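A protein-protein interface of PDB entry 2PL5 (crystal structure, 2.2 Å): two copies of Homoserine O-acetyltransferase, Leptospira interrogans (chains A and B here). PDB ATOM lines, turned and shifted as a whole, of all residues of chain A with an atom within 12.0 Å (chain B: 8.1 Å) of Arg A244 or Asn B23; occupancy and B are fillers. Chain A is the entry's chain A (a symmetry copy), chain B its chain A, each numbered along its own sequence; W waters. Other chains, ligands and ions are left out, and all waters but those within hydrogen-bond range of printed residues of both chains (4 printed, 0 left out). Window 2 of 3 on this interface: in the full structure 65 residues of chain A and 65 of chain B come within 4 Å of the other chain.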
ATOM      1  N   LYS A 237      11.592 -38.260 -14.251  1.00  0.00           N
ATOM      2  CA  LYS A 237      10.866 -37.239 -13.506  1.00  0.00           C
ATOM      3  C   LYS A 237      11.794 -36.163 -12.910  1.00  0.00           C
ATOM      4  O   LYS A 237      11.464 -34.985 -12.936  1.00  0.00           O
ATOM      5  CB  LYS A 237      10.008 -37.872 -12.400  1.00  0.00           C
ATOM      6  CG  LYS A 237       9.149 -36.850 -11.667  1.00  0.00           C
ATOM      7  CD  LYS A 237       8.171 -37.460 -10.667  1.00  0.00           C
ATOM      8  CE  LYS A 237       7.384 -36.334  -9.985  1.00  0.00           C
ATOM      9  NZ  LYS A 237       6.382 -36.811  -8.991  1.00  0.00           N
ATOM     10  N   PHE A 238      12.942 -36.571 -12.374  1.00  0.00           N
ATOM     11  CA  PHE A 238      13.827 -35.633 -11.674  1.00  0.00           C
ATOM     12  C   PHE A 238      14.883 -34.944 -12.559  1.00  0.00           C
ATOM     13  O   PHE A 238      15.325 -33.831 -12.254  1.00  0.00           O
ATOM     14  CB  PHE A 238      14.426 -36.271 -10.410  1.00  0.00           C
ATOM     15  CG  PHE A 238      13.507 -36.200  -9.216  1.00  0.00           C
ATOM     16  CD1 PHE A 238      12.408 -37.053  -9.108  1.00  0.00           C
ATOM     17  CD2 PHE A 238      13.717 -35.260  -8.213  1.00  0.00           C
ATOM     18  CE1 PHE A 238      11.537 -36.973  -8.010  1.00  0.00           C
ATOM     19  CE2 PHE A 238      12.857 -35.176  -7.121  1.00  0.00           C
ATOM     20  CZ  PHE A 238      11.764 -36.032  -7.017  1.00  0.00           C
ATOM     21  N   GLY A 239      15.258 -35.591 -13.661  1.00  0.00           N
ATOM     22  CA  GLY A 239      16.180 -34.994 -14.631  1.00  0.00           C
ATOM     23  C   GLY A 239      17.560 -34.742 -14.054  1.00  0.00           C
ATOM     24  O   GLY A 239      18.008 -35.467 -13.163  1.00  0.00           O
ATOM     25  N   ARG A 240      18.224 -33.706 -14.564  1.00  0.00           N
ATOM     26  CA  ARG A 240      19.600 -33.374 -14.173  1.00  0.00           C
ATOM     27  C   ARG A 240      19.690 -32.003 -13.491  1.00  0.00           C
ATOM     28  O   ARG A 240      20.785 -31.541 -13.141  1.00  0.00           O
ATOM     29  CB  ARG A 240      20.525 -33.389 -15.397  1.00  0.00           C
ATOM     30  CG  ARG A 240      20.647 -34.718 -16.120  1.00  0.00           C
ATOM     31  CD  ARG A 240      21.221 -34.491 -17.517  1.00  0.00           C
ATOM     32  NE  ARG A 240      20.330 -33.656 -18.329  1.00  0.00           N
ATOM     33  CZ  ARG A 240      20.639 -33.134 -19.515  1.00  0.00           C
ATOM     34  NH1 ARG A 240      21.833 -33.344 -20.057  1.00  0.00           N
ATOM     35  NH2 ARG A 240      19.746 -32.395 -20.160  1.00  0.00           N
ATOM     36  N   ASN A 241      18.536 -31.366 -13.299  1.00  0.00           N
ATOM     37  CA  ASN A 241      18.453 -30.026 -12.721  1.00  0.00           C
ATOM     38  C   ASN A 241      17.241 -29.864 -11.807  1.00  0.00           C
ATOM     39  O   ASN A 241      16.190 -30.429 -12.091  1.00  0.00           O
ATOM     40  CB  ASN A 241      18.388 -28.974 -13.833  1.00  0.00           C
ATOM     41  CG  ASN A 241      19.661 -28.909 -14.641  1.00  0.00           C
ATOM     42  OD1 ASN A 241      20.725 -28.548 -14.127  1.00  0.00           O
ATOM     43  ND2 ASN A 241      19.569 -29.280 -15.912  1.00  0.00           N
ATOM     44  N   PRO A 242      17.390 -29.101 -10.706  1.00  0.00           N
ATOM     45  CA  PRO A 242      16.264 -28.749  -9.835  1.00  0.00           C
ATOM     46  C   PRO A 242      15.382 -27.680 -10.490  1.00  0.00           C
ATOM     47  O   PRO A 242      15.753 -27.164 -11.544  1.00  0.00           O
ATOM     48  CB  PRO A 242      16.959 -28.210  -8.579  1.00  0.00           C
ATOM     49  CG  PRO A 242      18.224 -27.639  -9.079  1.00  0.00           C
ATOM     50  CD  PRO A 242      18.660 -28.542 -10.200  1.00  0.00           C
ATOM     51  N   PRO A 243      14.214 -27.361  -9.894  1.00  0.00           N
ATOM     52  CA  PRO A 243      13.309 -26.388 -10.526  1.00  0.00           C
ATOM     53  C   PRO A 243      13.846 -24.955 -10.601  1.00  0.00           C
ATOM     54  O   PRO A 243      14.787 -24.597  -9.887  1.00  0.00           O
ATOM     55  CB  PRO A 243      12.061 -26.418  -9.626  1.00  0.00           C
ATOM     56  CG  PRO A 243      12.194 -27.646  -8.796  1.00  0.00           C
ATOM     57  CD  PRO A 243      13.647 -27.898  -8.643  1.00  0.00           C
ATOM     58  N   ARG A 244      13.228 -24.151 -11.469  1.00  0.00           N
ATOM     59  CA  ARG A 244      13.485 -22.716 -11.539  1.00  0.00           C
ATOM     60  C   ARG A 244      12.776 -22.064 -10.361  1.00  0.00           C
ATOM     61  O   ARG A 244      11.843 -22.639  -9.805  1.00  0.00           O
ATOM     62  CB  ARG A 244      12.967 -22.128 -12.860  1.00  0.00           C
ATOM     63  CG  ARG A 244      13.327 -22.926 -14.117  1.00  0.00           C
ATOM     64  CD  ARG A 244      14.742 -22.654 -14.613  1.00  0.00           C
ATOM     65  NE  ARG A 244      14.828 -21.421 -15.395  1.00  0.00           N
ATOM     66  CZ  ARG A 244      15.889 -21.052 -16.110  1.00  0.00           C
ATOM     67  NH1 ARG A 244      16.974 -21.818 -16.156  1.00  0.00           N
ATOM     68  NH2 ARG A 244      15.866 -19.909 -16.782  1.00  0.00           N
ATOM     69  N   GLY A 245      13.221 -20.877  -9.968  1.00  0.00           N
ATOM     70  CA  GLY A 245      12.570 -20.142  -8.882  1.00  0.00           C
ATOM     71  C   GLY A 245      12.815 -20.680  -7.477  1.00  0.00           C
ATOM     72  O   GLY A 245      13.917 -21.118  -7.136  1.00  0.00           O
ATOM     73  N   ASN A 246      11.769 -20.629  -6.660  1.00  0.00           N
ATOM     74  CA  ASN A 246      11.840 -21.009  -5.253  1.00  0.00           C
ATOM     75  C   ASN A 246      10.664 -21.900  -4.849  1.00  0.00           C
ATOM     76  O   ASN A 246       9.818 -22.232  -5.686  1.00  0.00           O
ATOM     77  CB  ASN A 246      11.915 -19.754  -4.369  1.00  0.00           C
ATOM     78  CG  ASN A 246      10.744 -18.798  -4.590  1.00  0.00           C
ATOM     79  OD1 ASN A 246       9.586 -19.202  -4.599  1.00  0.00           O
ATOM     80  ND2 ASN A 246      11.051 -17.521  -4.749  1.00  0.00           N
ATOM     81  N   ILE A 247      10.606 -22.279  -3.573  1.00  0.00           N
ATOM     82  CA  ILE A 247       9.541 -23.160  -3.073  1.00  0.00           C
ATOM     83  C   ILE A 247       8.142 -22.533  -3.239  1.00  0.00           C
ATOM     84  O   ILE A 247       7.192 -23.226  -3.571  1.00  0.00           O
ATOM     85  CB  ILE A 247       9.824 -23.650  -1.618  1.00  0.00           C
ATOM     86  CG1 ILE A 247      10.974 -24.666  -1.623  1.00  0.00           C
ATOM     87  CG2 ILE A 247       8.577 -24.265  -0.982  1.00  0.00           C
ATOM     88  CD1 ILE A 247      11.447 -25.109  -0.236  1.00  0.00           C
ATOM     89  N   LEU A 248       8.043 -21.221  -3.043  1.00  0.00           N
ATOM     90  CA  LEU A 248       6.787 -20.483  -3.224  1.00  0.00           C
ATOM     91  C   LEU A 248       6.359 -20.336  -4.685  1.00  0.00           C
ATOM     92  O   LEU A 248       5.179 -20.492  -5.005  1.00  0.00           O
ATOM     93  CB  LEU A 248       6.909 -19.078  -2.631  1.00  0.00           C
ATOM     94  CG  LEU A 248       6.651 -18.787  -1.159  1.00  0.00           C
ATOM     95  CD1 LEU A 248       6.889 -17.314  -0.952  1.00  0.00           C
ATOM     96  CD2 LEU A 248       5.232 -19.152  -0.740  1.00  0.00           C
ATOM     97  N   SER A 249       7.320 -20.011  -5.553  1.00  0.00           N
ATOM     98  CA  SER A 249       7.065 -19.682  -6.960  1.00  0.00           C
ATOM     99  C   SER A 249       6.609 -20.866  -7.793  1.00  0.00           C
ATOM    100  O   SER A 249       5.719 -20.732  -8.631  1.00  0.00           O
ATOM    101  CB  SER A 249       8.307 -19.064  -7.606  1.00  0.00           C
ATOM    102  OG  SER A 249       8.527 -17.749  -7.123  1.00  0.00           O
ATOM    103  N   THR A 250       7.232 -22.017  -7.573  1.00  0.00           N
ATOM    104  CA  THR A 250       6.895 -23.233  -8.306  1.00  0.00           C
ATOM    105  C   THR A 250       5.598 -23.846  -7.788  1.00  0.00           C
ATOM    106  O   THR A 250       5.167 -24.905  -8.264  1.00  0.00           O
ATOM    107  CB  THR A 250       8.019 -24.283  -8.188  1.00  0.00           C
ATOM    108  OG1 THR A 250       8.496 -24.322  -6.835  1.00  0.00           O
ATOM    109  CG2 THR A 250       9.168 -23.945  -9.128  1.00  0.00           C
ATOM    110  N   ASP A 251       4.987 -23.169  -6.815  1.00  0.00           N
ATOM    111  CA  ASP A 251       3.814 -23.670  -6.096  1.00  0.00           C
ATOM    112  C   ASP A 251       4.150 -24.968  -5.367  1.00  0.00           C
ATOM    113  O   ASP A 251       3.256 -25.714  -4.958  1.00  0.00           O
ATOM    114  CB  ASP A 251       2.609 -23.844  -7.034  1.00  0.00           C
ATOM    115  CG  ASP A 251       2.087 -22.523  -7.563  1.00  0.00           C
ATOM    116  OD1 ASP A 251       1.928 -22.398  -8.796  1.00  0.00           O
ATOM    117  OD2 ASP A 251       1.843 -21.607  -6.749  1.00  0.00           O
ATOM    118  N   PHE A 252       5.452 -25.219  -5.213  1.00  0.00           N
ATOM    119  CA  PHE A 252       5.962 -26.336  -4.422  1.00  0.00           C
ATOM    120  C   PHE A 252       5.493 -26.200  -2.973  1.00  0.00           C
ATOM    121  O   PHE A 252       5.318 -27.201  -2.272  1.00  0.00           O
ATOM    122  CB  PHE A 252       7.494 -26.363  -4.478  1.00  0.00           C
ATOM    123  CG  PHE A 252       8.102 -27.666  -4.036  1.00  0.00           C
ATOM    124  CD1 PHE A 252       8.393 -28.659  -4.964  1.00  0.00           C
ATOM    125  CD2 PHE A 252       8.399 -27.894  -2.695  1.00  0.00           C
ATOM    126  CE1 PHE A 252       8.959 -29.863  -4.561  1.00  0.00           C
ATOM    127  CE2 PHE A 252       8.962 -29.093  -2.281  1.00  0.00           C
ATOM    128  CZ  PHE A 252       9.243 -30.082  -3.214  1.00  0.00           C
ATOM    129  N   ALA A 253       5.286 -24.951  -2.548  1.00  0.00           N
ATOM    130  CA  ALA A 253       4.811 -24.615  -1.205  1.00  0.00           C
ATOM    131  C   ALA A 253       3.416 -25.160  -0.912  1.00  0.00           C
ATOM    132  O   ALA A 253       3.149 -25.595   0.207  1.00  0.00           O
ATOM    133  CB  ALA A 253       4.847 -23.107  -1.000  1.00  0.00           C
ATOM    134  N   LEU B  20      26.198 -14.586  -6.487  1.00  0.00           N
ATOM    135  CA  LEU B  20      26.394 -15.844  -7.192  1.00  0.00           C
ATOM    136  C   LEU B  20      25.176 -16.074  -8.055  1.00  0.00           C
ATOM    137  O   LEU B  20      24.051 -16.160  -7.554  1.00  0.00           O
ATOM    138  CB  LEU B  20      26.608 -17.030  -6.236  1.00  0.00           C
ATOM    139  CG  LEU B  20      26.696 -18.422  -6.882  1.00  0.00           C
ATOM    140  CD1 LEU B  20      27.908 -18.532  -7.819  1.00  0.00           C
ATOM    141  CD2 LEU B  20      26.728 -19.529  -5.833  1.00  0.00           C
ATOM    142  N   ILE B  21      25.417 -16.153  -9.355  1.00  0.00           N
ATOM    143  CA  ILE B  21      24.369 -16.435 -10.314  1.00  0.00           C
ATOM    144  C   ILE B  21      24.184 -17.947 -10.360  1.00  0.00           C
ATOM    145  O   ILE B  21      25.126 -18.695 -10.640  1.00  0.00           O
ATOM    146  CB  ILE B  21      24.691 -15.831 -11.700  1.00  0.00           C
ATOM    147  CG1 ILE B  21      24.758 -14.299 -11.582  1.00  0.00           C
ATOM    148  CG2 ILE B  21      23.643 -16.241 -12.723  1.00  0.00           C
ATOM    149  CD1 ILE B  21      25.339 -13.576 -12.804  1.00  0.00           C
ATOM    150  N   LEU B  22      22.969 -18.383 -10.054  1.00  0.00           N
ATOM    151  CA  LEU B  22      22.674 -19.800  -9.943  1.00  0.00           C
ATOM    152  C   LEU B  22      22.296 -20.366 -11.296  1.00  0.00           C
ATOM    153  O   LEU B  22      21.924 -19.625 -12.207  1.00  0.00           O
ATOM    154  CB  LEU B  22      21.549 -20.036  -8.929  1.00  0.00           C
ATOM    155  CG  LEU B  22      21.783 -19.535  -7.503  1.00  0.00           C
ATOM    156  CD1 LEU B  22      20.504 -19.692  -6.693  1.00  0.00           C
ATOM    157  CD2 LEU B  22      22.955 -20.243  -6.832  1.00  0.00           C
ATOM    158  N   ASN B  23      22.396 -21.686 -11.417  1.00  0.00           N
ATOM    159  CA  ASN B  23      22.134 -22.375 -12.669  1.00  0.00           C
ATOM    160  C   ASN B  23      20.694 -22.225 -13.150  1.00  0.00           C
ATOM    161  O   ASN B  23      20.437 -22.297 -14.350  1.00  0.00           O
ATOM    162  CB  ASN B  23      22.502 -23.863 -12.547  1.00  0.00           C
ATOM    163  CG  ASN B  23      23.958 -24.152 -12.924  1.00  0.00           C
ATOM    164  OD1 ASN B  23      24.808 -23.256 -12.948  1.00  0.00           O
ATOM    165  ND2 ASN B  23      24.243 -25.414 -13.233  1.00  0.00           N
ATOM    166  N   ASN B  24      19.760 -22.019 -12.221  1.00  0.00           N
ATOM    167  CA  ASN B  24      18.343 -21.871 -12.582  1.00  0.00           C
ATOM    168  C   ASN B  24      17.929 -20.431 -12.925  1.00  0.00           C
ATOM    169  O   ASN B  24      16.738 -20.143 -13.099  1.00  0.00           O
ATOM    170  CB  ASN B  24      17.417 -22.502 -11.519  1.00  0.00           C
ATOM    171  CG  ASN B  24      17.278 -21.666 -10.249  1.00  0.00           C
ATOM    172  OD1 ASN B  24      16.452 -21.979  -9.382  1.00  0.00           O
ATOM    173  ND2 ASN B  24      18.071 -20.611 -10.125  1.00  0.00           N
ATOM    174  N   GLY B  25      18.916 -19.540 -13.018  1.00  0.00           N
ATOM    175  CA  GLY B  25      18.671 -18.130 -13.341  1.00  0.00           C
ATOM    176  C   GLY B  25      18.610 -17.173 -12.157  1.00  0.00           C
ATOM    177  O   GLY B  25      18.876 -15.978 -12.311  1.00  0.00           O
ATOM    178  N   SER B  26      18.250 -17.680 -10.978  1.00  0.00           N
ATOM    179  CA  SER B  26      18.177 -16.851  -9.771  1.00  0.00           C
ATOM    180  C   SER B  26      19.561 -16.404  -9.309  1.00  0.00           C
ATOM    181  O   SER B  26      20.571 -17.004  -9.674  1.00  0.00           O
ATOM    182  CB  SER B  26      17.456 -17.592  -8.641  1.00  0.00           C
ATOM    183  OG  SER B  26      16.108 -17.866  -8.975  1.00  0.00           O
ATOM    184  N   VAL B  27      19.599 -15.344  -8.509  1.00  0.00           N
ATOM    185  CA  VAL B  27      20.851 -14.747  -8.054  1.00  0.00           C
ATOM    186  C   VAL B  27      20.864 -14.653  -6.539  1.00  0.00           C
ATOM    187  O   VAL B  27      19.890 -14.203  -5.937  1.00  0.00           O
ATOM    188  CB  VAL B  27      21.054 -13.320  -8.664  1.00  0.00           C
ATOM    189  CG1 VAL B  27      22.350 -12.692  -8.179  1.00  0.00           C
ATOM    190  CG2 VAL B  27      21.037 -13.371 -10.197  1.00  0.00           C
ATOM    191  N   PHE B 122      13.818 -18.485  -0.713  1.00  0.00           N
ATOM    192  CA  PHE B 122      15.183 -18.800  -1.140  1.00  0.00           C
ATOM    193  C   PHE B 122      15.125 -19.583  -2.451  1.00  0.00           C
ATOM    194  O   PHE B 122      14.257 -20.434  -2.621  1.00  0.00           O
ATOM    195  CB  PHE B 122      15.932 -19.572  -0.037  1.00  0.00           C
ATOM    196  CG  PHE B 122      17.395 -19.800  -0.328  1.00  0.00           C
ATOM    197  CD1 PHE B 122      18.339 -18.824  -0.038  1.00  0.00           C
ATOM    198  CD2 PHE B 122      17.826 -20.998  -0.884  1.00  0.00           C
ATOM    199  CE1 PHE B 122      19.689 -19.033  -0.309  1.00  0.00           C
ATOM    200  CE2 PHE B 122      19.173 -21.222  -1.161  1.00  0.00           C
ATOM    201  CZ  PHE B 122      20.106 -20.232  -0.880  1.00  0.00           C
ATOM    202  N   PRO B 123      16.018 -19.267  -3.406  1.00  0.00           N
ATOM    203  CA  PRO B 123      16.000 -20.011  -4.668  1.00  0.00           C
ATOM    204  C   PRO B 123      16.464 -21.461  -4.536  1.00  0.00           C
ATOM    205  O   PRO B 123      17.309 -21.759  -3.694  1.00  0.00           O
ATOM    206  CB  PRO B 123      16.987 -19.243  -5.545  1.00  0.00           C
ATOM    207  CG  PRO B 123      17.858 -18.532  -4.612  1.00  0.00           C
ATOM    208  CD  PRO B 123      17.041 -18.202  -3.407  1.00  0.00           C
ATOM    209  N   PHE B 124      15.910 -22.343  -5.373  1.00  0.00           N
ATOM    210  CA  PHE B 124      16.438 -23.689  -5.526  1.00  0.00           C
ATOM    211  C   PHE B 124      17.897 -23.627  -5.942  1.00  0.00           C
ATOM    212  O   PHE B 124      18.282 -22.843  -6.828  1.00  0.00           O
ATOM    213  CB  PHE B 124      15.642 -24.509  -6.549  1.00  0.00           C
ATOM    214  CG  PHE B 124      14.334 -25.033  -6.022  1.00  0.00           C
ATOM    215  CD1 PHE B 124      13.141 -24.424  -6.375  1.00  0.00           C
ATOM    216  CD2 PHE B 124      14.300 -26.132  -5.155  1.00  0.00           C
ATOM    217  CE1 PHE B 124      11.924 -24.895  -5.878  1.00  0.00           C
ATOM    218  CE2 PHE B 124      13.094 -26.617  -4.661  1.00  0.00           C
ATOM    219  CZ  PHE B 124      11.902 -25.995  -5.017  1.00  0.00           C
ATOM    220  N   VAL B 125      18.692 -24.461  -5.283  1.00  0.00           N
ATOM    221  CA  VAL B 125      20.110 -24.609  -5.564  1.00  0.00           C
ATOM    222  C   VAL B 125      20.390 -26.036  -6.034  1.00  0.00           C
ATOM    223  O   VAL B 125      19.619 -26.960  -5.754  1.00  0.00           O
ATOM    224  CB  VAL B 125      20.990 -24.243  -4.330  1.00  0.00           C
ATOM    225  CG1 VAL B 125      20.945 -22.738  -4.063  1.00  0.00           C
ATOM    226  CG2 VAL B 125      20.572 -25.045  -3.076  1.00  0.00           C
ATOM    227  N   SER B 126      21.474 -26.190  -6.789  1.00  0.00           N
ATOM    228  CA  SER B 126      21.898 -27.465  -7.303  1.00  0.00           C
ATOM    229  C   SER B 126      23.252 -27.777  -6.704  1.00  0.00           C
ATOM    230  O   SER B 126      23.892 -26.909  -6.116  1.00  0.00           O
ATOM    231  CB  SER B 126      22.003 -27.412  -8.830  1.00  0.00           C
ATOM    232  OG  SER B 126      22.952 -26.425  -9.238  1.00  0.00           O
ATOM    233  N   ILE B 127      23.696 -29.018  -6.855  1.00  0.00           N
ATOM    234  CA  ILE B 127      25.068 -29.380  -6.485  1.00  0.00           C
ATOM    235  C   ILE B 127      26.108 -28.590  -7.312  1.00  0.00           C
ATOM    236  O   ILE B 127      27.161 -28.232  -6.799  1.00  0.00           O
ATOM    237  CB  ILE B 127      25.294 -30.908  -6.571  1.00  0.00           C
ATOM    238  CG1 ILE B 127      24.521 -31.606  -5.437  1.00  0.00           C
ATOM    239  CG2 ILE B 127      26.776 -31.251  -6.491  1.00  0.00           C
ATOM    240  CD1 ILE B 127      24.604 -33.101  -5.458  1.00  0.00           C
ATOM    241  N   GLN B 128      25.815 -28.313  -8.582  1.00  0.00           N
ATOM    242  CA  GLN B 128      26.738 -27.481  -9.366  1.00  0.00           C
ATOM    243  C   GLN B 128      26.900 -26.067  -8.775  1.00  0.00           C
ATOM    244  O   GLN B 128      28.025 -25.556  -8.705  1.00  0.00           O
ATOM    245  CB  GLN B 128      26.495 -27.513 -10.900  1.00  0.00           C
ATOM    246  CG  GLN B 128      25.101 -27.806 -11.386  1.00  0.00           C
ATOM    247  CD  GLN B 128      24.664 -29.268 -11.276  1.00  0.00           C
ATOM    248  OE1 GLN B 128      25.045 -30.132 -12.077  1.00  0.00           O
ATOM    249  NE2 GLN B 128      23.820 -29.530 -10.316  1.00  0.00           N
ATOM    250  N   ASP B 129      25.794 -25.485  -8.297  1.00  0.00           N
ATOM    251  CA  ASP B 129      25.803 -24.206  -7.559  1.00  0.00           C
ATOM    252  C   ASP B 129      26.615 -24.282  -6.272  1.00  0.00           C
ATOM    253  O   ASP B 129      27.403 -23.391  -5.972  1.00  0.00           O
ATOM    254  CB  ASP B 129      24.378 -23.754  -7.184  1.00  0.00           C
ATOM    255  CG  ASP B 129      23.498 -23.508  -8.387  1.00  0.00           C
ATOM    256  OD1 ASP B 129      23.994 -22.994  -9.412  1.00  0.00           O
ATOM    257  OD2 ASP B 129      22.298 -23.835  -8.304  1.00  0.00           O
ATOM    258  N   MET B 130      26.397 -25.338  -5.498  1.00  0.00           N
ATOM    259  CA  MET B 130      27.114 -25.529  -4.233  1.00  0.00           C
ATOM    260  C   MET B 130      28.626 -25.544  -4.451  1.00  0.00           C
ATOM    261  O   MET B 130      29.382 -24.984  -3.660  1.00  0.00           O
ATOM    262  CB  MET B 130      26.673 -26.829  -3.555  1.00  0.00           C
ATOM    263  CG  MET B 130      25.215 -26.847  -3.062  1.00  0.00           C
ATOM    264  SD  MET B 130      24.770 -28.494  -2.449  1.00  0.00           S
ATOM    265  CE  MET B 130      23.083 -28.184  -1.927  1.00  0.00           C
ATOM    266  N   LYS B 132      30.170 -24.221  -7.250  1.00  0.00           N
ATOM    267  CA  LYS B 132      30.524 -22.865  -7.717  1.00  0.00           C
ATOM    268  C   LYS B 132      30.835 -21.957  -6.540  1.00  0.00           C
ATOM    269  O   LYS B 132      31.784 -21.182  -6.575  1.00  0.00           O
ATOM    270  CB  LYS B 132      29.382 -22.235  -8.516  1.00  0.00           C
ATOM    271  CG  LYS B 132      29.641 -22.050 -10.002  1.00  0.00           C
ATOM    272  CD  LYS B 132      28.751 -20.945 -10.570  1.00  0.00           C
ATOM    273  CE  LYS B 132      29.544 -19.703 -10.967  1.00  0.00           C
ATOM    274  NZ  LYS B 132      29.807 -19.654 -12.440  1.00  0.00           N
ATOM    275  N   GLU B 161      31.358 -33.585  -8.547  1.00  0.00           N
ATOM    276  CA  GLU B 161      31.065 -32.376  -9.315  1.00  0.00           C
ATOM    277  C   GLU B 161      32.321 -31.512  -9.534  1.00  0.00           C
ATOM    278  O   GLU B 161      32.550 -31.042 -10.647  1.00  0.00           O
ATOM    279  CB  GLU B 161      29.905 -31.585  -8.681  1.00  0.00           C
ATOM    280  CG  GLU B 161      29.623 -30.198  -9.266  1.00  0.00           C
ATOM    281  CD  GLU B 161      29.202 -30.186 -10.733  1.00  0.00           C
ATOM    282  OE1 GLU B 161      28.795 -31.234 -11.280  1.00  0.00           O
ATOM    283  OE2 GLU B 161      29.285 -29.099 -11.346  1.00  0.00           O
HETATM  284  O   HOH W   1      21.495 -30.473 -10.710  1.00  0.00           O
HETATM  285  O   HOH W   2      23.005 -32.766 -12.878  1.00  0.00           O
HETATM  286  O   HOH W   3      15.050 -19.091 -11.259  1.00  0.00           O
HETATM  287  O   HOH W   4      22.281 -26.980 -12.219  1.00  0.00           O
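OD1 of Asn B24 is in hydrogen-bond range of N of Gly A245, 3.5 Å away.
O of Asn B24 is in hydrogen-bond range of NE of Arg A244.
The backbone NH of Phe B124 lies within hydrogen-bond range of the backbone carbonyl oxygen of Gly A245.
The side-chain amide oxygen (OD1) of Asn B24 lies close to the backbone carbonyl oxygen (O) of Pro A243, at 3.1 Å.
The backbone carbonyl oxygen of Ile A247 lies within hydrogen-bond range of the backbone NH of Phe A252 (3.1 Å).
The side-chain amide nitrogen (ND2) of Asn B24 sits close to the backbone NH (N) of Ser B26.
The side-chain amide oxygen of Asn A246 is in hydrogen-bond range of the backbone NH of Leu A248, at 3.0 Å.
The backbone NH (N) of Asn B23 sits at hydrogen-bond distance from the side-chain carboxylate (OD1) of Asp B129, at 2.9 Å.
The side-chain hydroxyl (OG) of Ser B126 sits close to the side-chain amide nitrogen (NE2) of Gln B128, at 3.4 Å.
O of Ile A247 sits at hydrogen-bond distance from N of Ala A253 (2.8 Å).
Among the printed residues, pairs that only touch across the chains: Pro A242 with Val B125 (3.7 Å), Pro A242 with Ser B126 (3.8 Å), Pro A243 with Phe B124 (3.4 Å), Arg A244 with Asn B23 (3.9 Å), Gly A245 with Pro B123 (3.4 Å), Asn A246 with Phe B122 (3.0 Å), Asn A246 with Phe B124 (3.4 Å), Ile A247 with Phe B124 (3.7 Å) and Thr A250 with Phe B124 (3.6 Å).
Arg A240 touches none of the printed residues of chain B.
Arg A244 touches two residues of chain B.
Of the printed residues of chain B, Asn A246 touches Phe B122 and Phe B124.
Leu A248 touches none of the printed residues of chain B.
Printed residues of chain B within 4 Å of Thr A250: Phe B124.
No residue of chain A comes within 4 Å of Leu B22.
Of chain A, only Pro A243 (3.1 Å), Arg A244 (3.2 Å) and Gly A245 (3.5 Å) come within 4 Å of Asn B24.
No residue of chain A comes within 4 Å of Ser B26.
Printed residues of chain A within 4 Å of Pro B123: Gly A245 (3.4 Å).
Of chain A, only Pro A243, Gly A245, Asn A246, Ile A247 and Thr A250 come within 4 Å of Phe B124.
Ser B126 touches one residue of chain A.
No residue of chain A comes within 4 Å of Asp B129.
The nearest residue of chain B that does not touch Arg A244 is Phe B124 (4.1 Å).
The nearest printed residue of chain B that does not touch Asn A246 is Pro B123 (4.1 Å).
Of the 17 printed residues of chain A, 7 touch a printed residue of chain B.
Of the 19 printed residues of chain B, 7 touch a printed residue of chain A.
Printed residues of chain B that touch a printed residue of chain A: Asn B23, Asn B24, Phe B122, Pro B123, Phe B124, Val B125 and Ser B126.
Hydrophobic or aromatic side chains of chain B within 4 Å of the printed part of chain A: Pro B123 and Phe B124.
Among the printed residues, 13 pairs touch across the chains.
No position is printed for both chains.
Water W1 lies within hydrogen-bond range of NE2 of Gln B128 (2.5 Å) and O of Arg A240 (2.7 Å).
Water W2 lies within hydrogen-bond range of the backbone carbonyl oxygen (O) of Arg A240 (2.5 Å) and the side-chain amide oxygen (OE1) of Gln B128 (3.4 Å).
Water W4 lies within hydrogen-bond range of ND2 of Asn B23 (2.7 Å), OD1 of Asn A241 (2.9 Å) and OG of Ser B126 (3.1 Å).
Water W3 lies within hydrogen-bond range of O of Asn B24 (2.7 Å), OG of Ser B26 (2.8 Å) and N of Gly A245 (2.9 Å).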
